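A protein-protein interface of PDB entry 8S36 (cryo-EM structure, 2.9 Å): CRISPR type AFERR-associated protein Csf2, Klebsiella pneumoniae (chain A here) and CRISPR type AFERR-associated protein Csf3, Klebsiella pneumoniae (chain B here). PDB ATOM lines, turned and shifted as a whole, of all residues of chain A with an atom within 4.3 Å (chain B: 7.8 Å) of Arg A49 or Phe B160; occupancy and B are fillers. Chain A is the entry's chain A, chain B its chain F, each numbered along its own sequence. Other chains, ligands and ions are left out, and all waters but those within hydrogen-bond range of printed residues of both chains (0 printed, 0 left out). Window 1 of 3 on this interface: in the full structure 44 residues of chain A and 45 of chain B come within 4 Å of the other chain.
The side-chain hydroxyl (OG1) of Thr A46 lies within hydrogen-bond range of the backbone carbonyl oxygen (O) of Ala B162. O of Gly A126 sits at hydrogen-bond distance from NE2 of His B152, at 2.8 Å. The backbone carbonyl oxygen of Val A125 sits close to the backbone carbonyl oxygen of Phe B160 (3.3 Å). The side-chain amino group of Lys A255 is in salt-bridge range of the side-chain carboxylate of Glu B32, at 3.6 Å.
NH2 of Arg A49 sits at hydrogen-bond distance from O of Val A125 (2.6 Å). O of Lys A124 sits at hydrogen-bond distance from N of Lys A255, at 3.0 Å. The backbone carbonyl oxygen of Leu A115 sits at hydrogen-bond distance from the backbone NH of Lys A124, at 2.7 Å. A ring nitrogen (ND1) of His B152 sits close to the side-chain hydroxyl (OH) of Tyr B159 (3.2 Å). OG of Ser B161 sits at hydrogen-bond distance from NH1 of Arg B85 (3.4 Å). The side-chain amide nitrogen (NE2) of Gln B36 sits at hydrogen-bond distance from the backbone carbonyl oxygen (O) of His B152, 3.0 Å away.
CG2 of Thr A46 touches NE of Arg B85, at 3.1 Å. Arg A49 touches Ser B161. Gly A123 touches Phe B160 (O to CE2, 3.7 Å). Lys A124 touches Phe B160. Gly A126 touches Phe B160 (CA to O, 3.0 Å). His B152 touches Ile A127. Ile A127 touches Ala B163 (O to CB, 3.3 Å). CB of His B152 touches CB of Ser A253, at 3.3 Å. Phe B160 touches Ser A253 (CZ to O, 3.9 Å). Lys A255 touches Phe B160 (CG to CZ, 3.4 Å).
Of chain B, only Phe B160 (3.9 Å) and Ser B161 (3.1 Å) come within 4 Å of Arg A49. Phe B160 touches just these residues of chain A: Arg A49, Gly A123, Lys A124, Val A125, Gly A126, Ser A253 and Lys A255. Of the printed residues of chain B, Lys A124 touches Phe B160. Of the printed residues of chain B, Lys A255 touches Glu B32, Gln B36 and Phe B160. Lys B93 touches none of the printed residues of chain A.
Of the 16 printed residues of chain B, 8 touch a printed residue of chain A. Hydrophobic or aromatic side chains of chain B within 4 Å of the printed part of chain A: His B152, Phe B160 and Ala B163. Of the 18 printed residues of chain A, 10 touch a printed residue of chain B. Along chain A the printed residues that touch a printed residue of chain B span positions 45 to 255. Among the printed residues, 17 pairs touch across the chains. Among the printed residues, Asp or Glu carboxylates within 4 Å of a Lys or Arg side-chain nitrogen of the other chain: Lys A255 with Glu B32 (3.6 Å).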
ATOM      1  N   GLY A  45     -11.680 -10.958  -2.486  1.00  0.00           N
ATOM      2  CA  GLY A  45     -10.324 -10.866  -2.985  1.00  0.00           C
ATOM      3  C   GLY A  45     -10.225 -11.112  -4.472  1.00  0.00           C
ATOM      4  O   GLY A  45      -9.217 -10.749  -5.085  1.00  0.00           O
ATOM      5  N   THR A  46     -11.260 -11.705  -5.069  1.00  0.00           N
ATOM      6  CA  THR A  46     -11.248 -11.941  -6.506  1.00  0.00           C
ATOM      7  C   THR A  46     -11.339 -10.632  -7.276  1.00  0.00           C
ATOM      8  O   THR A  46     -10.642 -10.450  -8.279  1.00  0.00           O
ATOM      9  CB  THR A  46     -12.400 -12.864  -6.899  1.00  0.00           C
ATOM     10  OG1 THR A  46     -12.375 -14.039  -6.080  1.00  0.00           O
ATOM     11  CG2 THR A  46     -12.276 -13.264  -8.359  1.00  0.00           C
ATOM     12  N   SER A  47     -12.203  -9.715  -6.839  1.00  0.00           N
ATOM     13  CA  SER A  47     -12.324  -8.441  -7.540  1.00  0.00           C
ATOM     14  C   SER A  47     -11.033  -7.641  -7.444  1.00  0.00           C
ATOM     15  O   SER A  47     -10.575  -7.064  -8.437  1.00  0.00           O
ATOM     16  CB  SER A  47     -13.492  -7.638  -6.972  1.00  0.00           C
ATOM     17  OG  SER A  47     -13.635  -6.403  -7.650  1.00  0.00           O
ATOM     18  N   ILE A  48     -10.422  -7.606  -6.258  1.00  0.00           N
ATOM     19  CA  ILE A  48      -9.159  -6.892  -6.106  1.00  0.00           C
ATOM     20  C   ILE A  48      -8.074  -7.564  -6.934  1.00  0.00           C
ATOM     21  O   ILE A  48      -7.229  -6.894  -7.539  1.00  0.00           O
ATOM     22  CB  ILE A  48      -8.759  -6.792  -4.621  1.00  0.00           C
ATOM     23  CG1 ILE A  48      -9.859  -6.113  -3.799  1.00  0.00           C
ATOM     24  CG2 ILE A  48      -7.464  -5.998  -4.479  1.00  0.00           C
ATOM     25  CD1 ILE A  48      -9.733  -6.344  -2.309  1.00  0.00           C
ATOM     26  N   ARG A  49      -8.073  -8.899  -6.973  1.00  0.00           N
ATOM     27  CA  ARG A  49      -7.067  -9.610  -7.754  1.00  0.00           C
ATOM     28  C   ARG A  49      -7.222  -9.319  -9.237  1.00  0.00           C
ATOM     29  O   ARG A  49      -6.231  -9.115  -9.944  1.00  0.00           O
ATOM     30  CB  ARG A  49      -7.171 -11.111  -7.496  1.00  0.00           C
ATOM     31  CG  ARG A  49      -6.094 -11.938  -8.183  1.00  0.00           C
ATOM     32  CD  ARG A  49      -6.190 -13.399  -7.783  1.00  0.00           C
ATOM     33  NE  ARG A  49      -4.883 -14.041  -7.720  1.00  0.00           N
ATOM     34  CZ  ARG A  49      -4.177 -14.416  -8.778  1.00  0.00           C
ATOM     35  NH1 ARG A  49      -4.620 -14.227 -10.010  1.00  0.00           N
ATOM     36  NH2 ARG A  49      -2.995 -14.998  -8.595  1.00  0.00           N
ATOM     37  N   GLY A  50      -8.459  -9.283  -9.725  1.00  0.00           N
ATOM     38  CA  GLY A  50      -8.684  -8.932 -11.116  1.00  0.00           C
ATOM     39  C   GLY A  50      -8.283  -7.503 -11.421  1.00  0.00           C
ATOM     40  O   GLY A  50      -7.702  -7.224 -12.472  1.00  0.00           O
ATOM     41  N   THR A  51      -8.592  -6.578 -10.512  1.00  0.00           N
ATOM     42  CA  THR A  51      -8.202  -5.187 -10.718  1.00  0.00           C
ATOM     43  C   THR A  51      -6.686  -5.048 -10.769  1.00  0.00           C
ATOM     44  O   THR A  51      -6.147  -4.341 -11.629  1.00  0.00           O
ATOM     45  CB  THR A  51      -8.782  -4.307  -9.612  1.00  0.00           C
ATOM     46  OG1 THR A  51     -10.186  -4.565  -9.477  1.00  0.00           O
ATOM     47  CG2 THR A  51      -8.570  -2.835  -9.932  1.00  0.00           C
ATOM     48  N   LEU A  52      -5.978  -5.735  -9.872  1.00  0.00           N
ATOM     49  CA  LEU A  52      -4.525  -5.638  -9.860  1.00  0.00           C
ATOM     50  C   LEU A  52      -3.911  -6.376 -11.041  1.00  0.00           C
ATOM     51  O   LEU A  52      -2.862  -5.967 -11.543  1.00  0.00           O
ATOM     52  CB  LEU A  52      -3.970  -6.186  -8.545  1.00  0.00           C
ATOM     53  CG  LEU A  52      -4.300  -5.417  -7.261  1.00  0.00           C
ATOM     54  CD1 LEU A  52      -3.491  -5.971  -6.102  1.00  0.00           C
ATOM     55  CD2 LEU A  52      -4.051  -3.923  -7.405  1.00  0.00           C
ATOM     56  N   ARG A  53      -4.570  -7.425 -11.535  1.00  0.00           N
ATOM     57  CA  ARG A  53      -4.079  -8.102 -12.727  1.00  0.00           C
ATOM     58  C   ARG A  53      -4.266  -7.226 -13.956  1.00  0.00           C
ATOM     59  O   ARG A  53      -3.398  -7.178 -14.832  1.00  0.00           O
ATOM     60  CB  ARG A  53      -4.798  -9.438 -12.909  1.00  0.00           C
ATOM     61  CG  ARG A  53      -4.452 -10.150 -14.204  1.00  0.00           C
ATOM     62  CD  ARG A  53      -4.775 -11.632 -14.132  1.00  0.00           C
ATOM     63  NE  ARG A  53      -4.292 -12.346 -15.309  1.00  0.00           N
ATOM     64  CZ  ARG A  53      -3.963 -13.631 -15.338  1.00  0.00           C
ATOM     65  NH1 ARG A  53      -4.067 -14.400 -14.265  1.00  0.00           N
ATOM     66  NH2 ARG A  53      -3.520 -14.161 -16.473  1.00  0.00           N
ATOM     67  N   LEU A 115       3.415 -13.758 -11.491  1.00  0.00           N
ATOM     68  CA  LEU A 115       2.606 -13.226 -10.399  1.00  0.00           C
ATOM     69  C   LEU A 115       1.192 -13.789 -10.448  1.00  0.00           C
ATOM     70  O   LEU A 115       0.754 -14.495  -9.532  1.00  0.00           O
ATOM     71  CB  LEU A 115       2.568 -11.699 -10.471  1.00  0.00           C
ATOM     72  CG  LEU A 115       3.882 -10.960 -10.229  1.00  0.00           C
ATOM     73  CD1 LEU A 115       3.761  -9.514 -10.683  1.00  0.00           C
ATOM     74  CD2 LEU A 115       4.271 -11.034  -8.763  1.00  0.00           C
ATOM     75  N   PHE A 116       0.479 -13.516 -11.536  1.00  0.00           N
ATOM     76  CA  PHE A 116      -0.870 -14.019 -11.759  1.00  0.00           C
ATOM     77  C   PHE A 116      -0.760 -15.165 -12.753  1.00  0.00           C
ATOM     78  O   PHE A 116      -0.455 -14.943 -13.928  1.00  0.00           O
ATOM     79  CB  PHE A 116      -1.797 -12.927 -12.294  1.00  0.00           C
ATOM     80  CG  PHE A 116      -1.725 -11.632 -11.535  1.00  0.00           C
ATOM     81  CD1 PHE A 116      -0.716 -10.717 -11.785  1.00  0.00           C
ATOM     82  CD2 PHE A 116      -2.684 -11.319 -10.587  1.00  0.00           C
ATOM     83  CE1 PHE A 116      -0.655  -9.525 -11.092  1.00  0.00           C
ATOM     84  CE2 PHE A 116      -2.627 -10.128  -9.892  1.00  0.00           C
ATOM     85  CZ  PHE A 116      -1.612  -9.230 -10.146  1.00  0.00           C
ATOM     86  N   GLY A 123      -0.116 -19.375  -9.966  1.00  0.00           N
ATOM     87  CA  GLY A 123       0.393 -18.030  -9.829  1.00  0.00           C
ATOM     88  C   GLY A 123       1.170 -17.859  -8.544  1.00  0.00           C
ATOM     89  O   GLY A 123       1.208 -18.743  -7.688  1.00  0.00           O
ATOM     90  N   LYS A 124       1.800 -16.692  -8.414  1.00  0.00           N
ATOM     91  CA  LYS A 124       2.579 -16.374  -7.229  1.00  0.00           C
ATOM     92  C   LYS A 124       2.023 -15.218  -6.414  1.00  0.00           C
ATOM     93  O   LYS A 124       2.550 -14.954  -5.329  1.00  0.00           O
ATOM     94  CB  LYS A 124       4.030 -16.050  -7.620  1.00  0.00           C
ATOM     95  CG  LYS A 124       4.729 -17.179  -8.363  1.00  0.00           C
ATOM     96  CD  LYS A 124       6.124 -17.444  -7.820  1.00  0.00           C
ATOM     97  CE  LYS A 124       7.071 -16.295  -8.125  1.00  0.00           C
ATOM     98  NZ  LYS A 124       8.492 -16.737  -8.137  1.00  0.00           N
ATOM     99  N   VAL A 125       0.976 -14.539  -6.878  1.00  0.00           N
ATOM    100  CA  VAL A 125       0.366 -13.430  -6.150  1.00  0.00           C
ATOM    101  C   VAL A 125      -0.977 -13.894  -5.598  1.00  0.00           C
ATOM    102  O   VAL A 125      -1.867 -14.304  -6.353  1.00  0.00           O
ATOM    103  CB  VAL A 125       0.221 -12.179  -7.033  1.00  0.00           C
ATOM    104  CG1 VAL A 125      -0.835 -12.366  -8.107  1.00  0.00           C
ATOM    105  CG2 VAL A 125      -0.092 -10.960  -6.180  1.00  0.00           C
ATOM    106  N   GLY A 126      -1.103 -13.864  -4.275  1.00  0.00           N
ATOM    107  CA  GLY A 126      -2.335 -14.157  -3.580  1.00  0.00           C
ATOM    108  C   GLY A 126      -2.960 -12.931  -2.956  1.00  0.00           C
ATOM    109  O   GLY A 126      -2.414 -12.368  -2.007  1.00  0.00           O
ATOM    110  N   ILE A 127      -4.097 -12.509  -3.488  1.00  0.00           N
ATOM    111  CA  ILE A 127      -4.803 -11.326  -3.017  1.00  0.00           C
ATOM    112  C   ILE A 127      -5.916 -11.780  -2.089  1.00  0.00           C
ATOM    113  O   ILE A 127      -6.542 -12.822  -2.318  1.00  0.00           O
ATOM    114  CB  ILE A 127      -5.366 -10.520  -4.202  1.00  0.00           C
ATOM    115  CG1 ILE A 127      -4.282 -10.285  -5.262  1.00  0.00           C
ATOM    116  CG2 ILE A 127      -5.964  -9.203  -3.740  1.00  0.00           C
ATOM    117  CD1 ILE A 127      -2.973  -9.756  -4.719  1.00  0.00           C
ATOM    118  N   SER A 253      -0.043 -11.242  -0.809  1.00  0.00           N
ATOM    119  CA  SER A 253       1.251 -11.881  -0.615  1.00  0.00           C
ATOM    120  C   SER A 253       1.788 -12.381  -1.942  1.00  0.00           C
ATOM    121  O   SER A 253       1.068 -13.043  -2.688  1.00  0.00           O
ATOM    122  CB  SER A 253       1.144 -13.042   0.374  1.00  0.00           C
ATOM    123  OG  SER A 253       2.357 -13.769   0.435  1.00  0.00           O
ATOM    124  N   LYS A 255       4.467 -15.043  -3.056  1.00  0.00           N
ATOM    125  CA  LYS A 255       5.252 -16.132  -2.491  1.00  0.00           C
ATOM    126  C   LYS A 255       6.432 -16.455  -3.393  1.00  0.00           C
ATOM    127  O   LYS A 255       6.288 -16.535  -4.616  1.00  0.00           O
ATOM    128  CB  LYS A 255       4.382 -17.377  -2.284  1.00  0.00           C
ATOM    129  CG  LYS A 255       4.023 -18.149  -3.553  1.00  0.00           C
ATOM    130  CD  LYS A 255       3.186 -19.380  -3.228  1.00  0.00           C
ATOM    131  CE  LYS A 255       4.033 -20.491  -2.626  1.00  0.00           C
ATOM    132  NZ  LYS A 255       3.331 -21.804  -2.648  1.00  0.00           N
ATOM    133  N   GLU B  32       1.492 -24.858   3.209  1.00  0.00           N
ATOM    134  CA  GLU B  32       1.490 -23.650   2.390  1.00  0.00           C
ATOM    135  C   GLU B  32       2.191 -22.514   3.124  1.00  0.00           C
ATOM    136  O   GLU B  32       2.985 -21.763   2.535  1.00  0.00           O
ATOM    137  CB  GLU B  32       0.055 -23.263   2.028  1.00  0.00           C
ATOM    138  CG  GLU B  32      -0.077 -22.037   1.127  1.00  0.00           C
ATOM    139  CD  GLU B  32       0.339 -22.311  -0.306  1.00  0.00           C
ATOM    140  OE1 GLU B  32       0.916 -23.387  -0.568  1.00  0.00           O
ATOM    141  OE2 GLU B  32       0.090 -21.447  -1.172  1.00  0.00           O
ATOM    142  N   GLN B  36       5.710 -20.607   2.098  1.00  0.00           N
ATOM    143  CA  GLN B  36       5.934 -19.175   1.967  1.00  0.00           C
ATOM    144  C   GLN B  36       7.059 -18.701   2.886  1.00  0.00           C
ATOM    145  O   GLN B  36       7.991 -18.034   2.427  1.00  0.00           O
ATOM    146  CB  GLN B  36       4.644 -18.414   2.280  1.00  0.00           C
ATOM    147  CG  GLN B  36       3.593 -18.500   1.189  1.00  0.00           C
ATOM    148  CD  GLN B  36       2.226 -18.052   1.665  1.00  0.00           C
ATOM    149  OE1 GLN B  36       2.111 -17.225   2.568  1.00  0.00           O
ATOM    150  NE2 GLN B  36       1.180 -18.597   1.056  1.00  0.00           N
ATOM    151  N   ARG B  85     -16.167 -17.398  -9.608  1.00  0.00           N
ATOM    152  CA  ARG B  85     -15.163 -16.681 -10.381  1.00  0.00           C
ATOM    153  C   ARG B  85     -15.753 -16.358 -11.746  1.00  0.00           C
ATOM    154  O   ARG B  85     -16.173 -17.264 -12.473  1.00  0.00           O
ATOM    155  CB  ARG B  85     -13.889 -17.512 -10.534  1.00  0.00           C
ATOM    156  CG  ARG B  85     -13.271 -17.970  -9.221  1.00  0.00           C
ATOM    157  CD  ARG B  85     -12.693 -16.809  -8.437  1.00  0.00           C
ATOM    158  NE  ARG B  85     -11.618 -16.136  -9.160  1.00  0.00           N
ATOM    159  CZ  ARG B  85     -10.351 -16.529  -9.171  1.00  0.00           C
ATOM    160  NH1 ARG B  85      -9.957 -17.618  -8.534  1.00  0.00           N
ATOM    161  NH2 ARG B  85      -9.456 -15.807  -9.837  1.00  0.00           N
ATOM    162  N   LYS B  93     -10.245  -3.767 -21.346  1.00  0.00           N
ATOM    163  CA  LYS B  93      -9.642  -5.021 -21.779  1.00  0.00           C
ATOM    164  C   LYS B  93      -9.978  -5.304 -23.236  1.00  0.00           C
ATOM    165  O   LYS B  93      -9.156  -5.857 -23.975  1.00  0.00           O
ATOM    166  CB  LYS B  93     -10.124  -6.170 -20.894  1.00  0.00           C
ATOM    167  CG  LYS B  93      -9.362  -6.323 -19.594  1.00  0.00           C
ATOM    168  CD  LYS B  93      -9.818  -7.559 -18.838  1.00  0.00           C
ATOM    169  CE  LYS B  93      -9.088  -7.710 -17.515  1.00  0.00           C
ATOM    170  NZ  LYS B  93      -9.482  -8.956 -16.803  1.00  0.00           N
ATOM    171  N   ALA B 151       0.753 -15.180   7.645  1.00  0.00           N
ATOM    172  CA  ALA B 151       1.030 -15.771   6.347  1.00  0.00           C
ATOM    173  C   ALA B 151      -0.252 -15.767   5.528  1.00  0.00           C
ATOM    174  O   ALA B 151      -1.357 -15.696   6.068  1.00  0.00           O
ATOM    175  CB  ALA B 151       1.576 -17.199   6.467  1.00  0.00           C
ATOM    176  N   HIS B 152      -0.087 -15.847   4.210  1.00  0.00           N
ATOM    177  CA  HIS B 152      -1.222 -15.837   3.290  1.00  0.00           C
ATOM    178  C   HIS B 152      -1.709 -17.266   3.054  1.00  0.00           C
ATOM    179  O   HIS B 152      -1.544 -17.853   1.984  1.00  0.00           O
ATOM    180  CB  HIS B 152      -0.844 -15.148   1.989  1.00  0.00           C
ATOM    181  CG  HIS B 152      -2.018 -14.619   1.229  1.00  0.00           C
ATOM    182  ND1 HIS B 152      -2.812 -13.598   1.705  1.00  0.00           N
ATOM    183  CD2 HIS B 152      -2.540 -14.975   0.031  1.00  0.00           C
ATOM    184  CE1 HIS B 152      -3.770 -13.345   0.830  1.00  0.00           C
ATOM    185  NE2 HIS B 152      -3.627 -14.167  -0.193  1.00  0.00           N
ATOM    186  N   VAL B 153      -2.323 -17.822   4.093  1.00  0.00           N
ATOM    187  CA  VAL B 153      -2.940 -19.139   4.026  1.00  0.00           C
ATOM    188  C   VAL B 153      -4.404 -19.010   4.411  1.00  0.00           C
ATOM    189  O   VAL B 153      -4.748 -18.308   5.368  1.00  0.00           O
ATOM    190  CB  VAL B 153      -2.224 -20.159   4.936  1.00  0.00           C
ATOM    191  CG1 VAL B 153      -0.857 -20.502   4.368  1.00  0.00           C
ATOM    192  CG2 VAL B 153      -2.102 -19.627   6.360  1.00  0.00           C
ATOM    193  N   GLY B 154      -5.259 -19.687   3.655  1.00  0.00           N
ATOM    194  CA  GLY B 154      -6.669 -19.784   3.960  1.00  0.00           C
ATOM    195  C   GLY B 154      -7.063 -21.236   4.079  1.00  0.00           C
ATOM    196  O   GLY B 154      -6.197 -22.115   4.047  1.00  0.00           O
ATOM    197  N   TYR B 157     -10.207 -24.332  -0.864  1.00  0.00           N
ATOM    198  CA  TYR B 157      -9.545 -24.371  -2.158  1.00  0.00           C
ATOM    199  C   TYR B 157      -9.300 -22.944  -2.640  1.00  0.00           C
ATOM    200  O   TYR B 157      -9.965 -22.003  -2.199  1.00  0.00           O
ATOM    201  CB  TYR B 157     -10.382 -25.198  -3.163  1.00  0.00           C
ATOM    202  CG  TYR B 157     -10.030 -25.017  -4.620  1.00  0.00           C
ATOM    203  CD1 TYR B 157      -8.810 -25.452  -5.112  1.00  0.00           C
ATOM    204  CD2 TYR B 157     -10.931 -24.464  -5.513  1.00  0.00           C
ATOM    205  CE1 TYR B 157      -8.483 -25.296  -6.442  1.00  0.00           C
ATOM    206  CE2 TYR B 157     -10.622 -24.323  -6.849  1.00  0.00           C
ATOM    207  CZ  TYR B 157      -9.396 -24.738  -7.308  1.00  0.00           C
ATOM    208  OH  TYR B 157      -9.078 -24.589  -8.637  1.00  0.00           O
ATOM    209  N   ASP B 158      -8.291 -22.799  -3.497  1.00  0.00           N
ATOM    210  CA  ASP B 158      -7.869 -21.565  -4.190  1.00  0.00           C
ATOM    211  C   ASP B 158      -7.958 -20.360  -3.261  1.00  0.00           C
ATOM    212  O   ASP B 158      -8.650 -19.380  -3.540  1.00  0.00           O
ATOM    213  CB  ASP B 158      -8.608 -21.211  -5.503  1.00  0.00           C
ATOM    214  CG  ASP B 158     -10.102 -21.499  -5.531  1.00  0.00           C
ATOM    215  OD1 ASP B 158     -10.703 -21.189  -6.581  1.00  0.00           O
ATOM    216  OD2 ASP B 158     -10.738 -21.866  -4.544  1.00  0.00           O
ATOM    217  N   TYR B 159      -7.262 -20.431  -2.131  1.00  0.00           N
ATOM    218  CA  TYR B 159      -7.174 -19.210  -1.348  1.00  0.00           C
ATOM    219  C   TYR B 159      -6.106 -18.293  -1.915  1.00  0.00           C
ATOM    220  O   TYR B 159      -6.248 -17.067  -1.859  1.00  0.00           O
ATOM    221  CB  TYR B 159      -6.862 -19.510   0.114  1.00  0.00           C
ATOM    222  CG  TYR B 159      -6.463 -18.270   0.874  1.00  0.00           C
ATOM    223  CD1 TYR B 159      -7.435 -17.429   1.387  1.00  0.00           C
ATOM    224  CD2 TYR B 159      -5.129 -17.934   1.082  1.00  0.00           C
ATOM    225  CE1 TYR B 159      -7.104 -16.300   2.076  1.00  0.00           C
ATOM    226  CE2 TYR B 159      -4.785 -16.791   1.778  1.00  0.00           C
ATOM    227  CZ  TYR B 159      -5.779 -15.979   2.274  1.00  0.00           C
ATOM    228  OH  TYR B 159      -5.452 -14.841   2.968  1.00  0.00           O
ATOM    229  N   PHE B 160      -5.036 -18.870  -2.459  1.00  0.00           N
ATOM    230  CA  PHE B 160      -4.012 -18.070  -3.112  1.00  0.00           C
ATOM    231  C   PHE B 160      -4.513 -17.373  -4.369  1.00  0.00           C
ATOM    232  O   PHE B 160      -3.851 -16.447  -4.840  1.00  0.00           O
ATOM    233  CB  PHE B 160      -2.799 -18.943  -3.440  1.00  0.00           C
ATOM    234  CG  PHE B 160      -1.491 -18.213  -3.348  1.00  0.00           C
ATOM    235  CD1 PHE B 160      -1.023 -17.753  -2.128  1.00  0.00           C
ATOM    236  CD2 PHE B 160      -0.723 -17.997  -4.477  1.00  0.00           C
ATOM    237  CE1 PHE B 160       0.178 -17.081  -2.039  1.00  0.00           C
ATOM    238  CE2 PHE B 160       0.480 -17.329  -4.392  1.00  0.00           C
ATOM    239  CZ  PHE B 160       0.931 -16.870  -3.172  1.00  0.00           C
ATOM    240  N   SER B 161      -5.616 -17.822  -4.967  1.00  0.00           N
ATOM    241  CA  SER B 161      -6.217 -17.100  -6.087  1.00  0.00           C
ATOM    242  C   SER B 161      -7.587 -16.522  -5.767  1.00  0.00           C
ATOM    243  O   SER B 161      -7.805 -15.321  -5.954  1.00  0.00           O
ATOM    244  CB  SER B 161      -6.304 -18.007  -7.323  1.00  0.00           C
ATOM    245  OG  SER B 161      -7.183 -19.089  -7.120  1.00  0.00           O
ATOM    246  N   ALA B 162      -8.522 -17.336  -5.282  1.00  0.00           N
ATOM    247  CA  ALA B 162      -9.888 -16.880  -5.064  1.00  0.00           C
ATOM    248  C   ALA B 162     -10.111 -16.287  -3.681  1.00  0.00           C
ATOM    249  O   ALA B 162     -11.231 -15.856  -3.385  1.00  0.00           O
ATOM    250  CB  ALA B 162     -10.866 -18.040  -5.268  1.00  0.00           C
ATOM    251  N   ALA B 163      -9.077 -16.232  -2.842  1.00  0.00           N
ATOM    252  CA  ALA B 163      -9.203 -15.749  -1.468  1.00  0.00           C
ATOM    253  C   ALA B 163     -10.378 -16.409  -0.756  1.00  0.00           C
ATOM    254  O   ALA B 163     -11.073 -15.787   0.049  1.00  0.00           O
ATOM    255  CB  ALA B 163      -9.348 -14.229  -1.436  1.00  0.00           C
ATOM    256  N   ASN B 164     -10.602 -17.686  -1.048  1.00  0.00           N
ATOM    257  CA  ASN B 164     -11.663 -18.429  -0.388  1.00  0.00           C
ATOM    258  C   ASN B 164     -11.176 -18.899   0.973  1.00  0.00           C
ATOM    259  O   ASN B 164     -10.019 -19.298   1.131  1.00  0.00           O
ATOM    260  CB  ASN B 164     -12.097 -19.627  -1.234  1.00  0.00           C
ATOM    261  CG  ASN B 164     -12.687 -19.232  -2.589  1.00  0.00           C
ATOM    262  OD1 ASN B 164     -12.652 -20.025  -3.529  1.00  0.00           O
ATOM    263  ND2 ASN B 164     -13.236 -18.022  -2.696  1.00  0.00           N
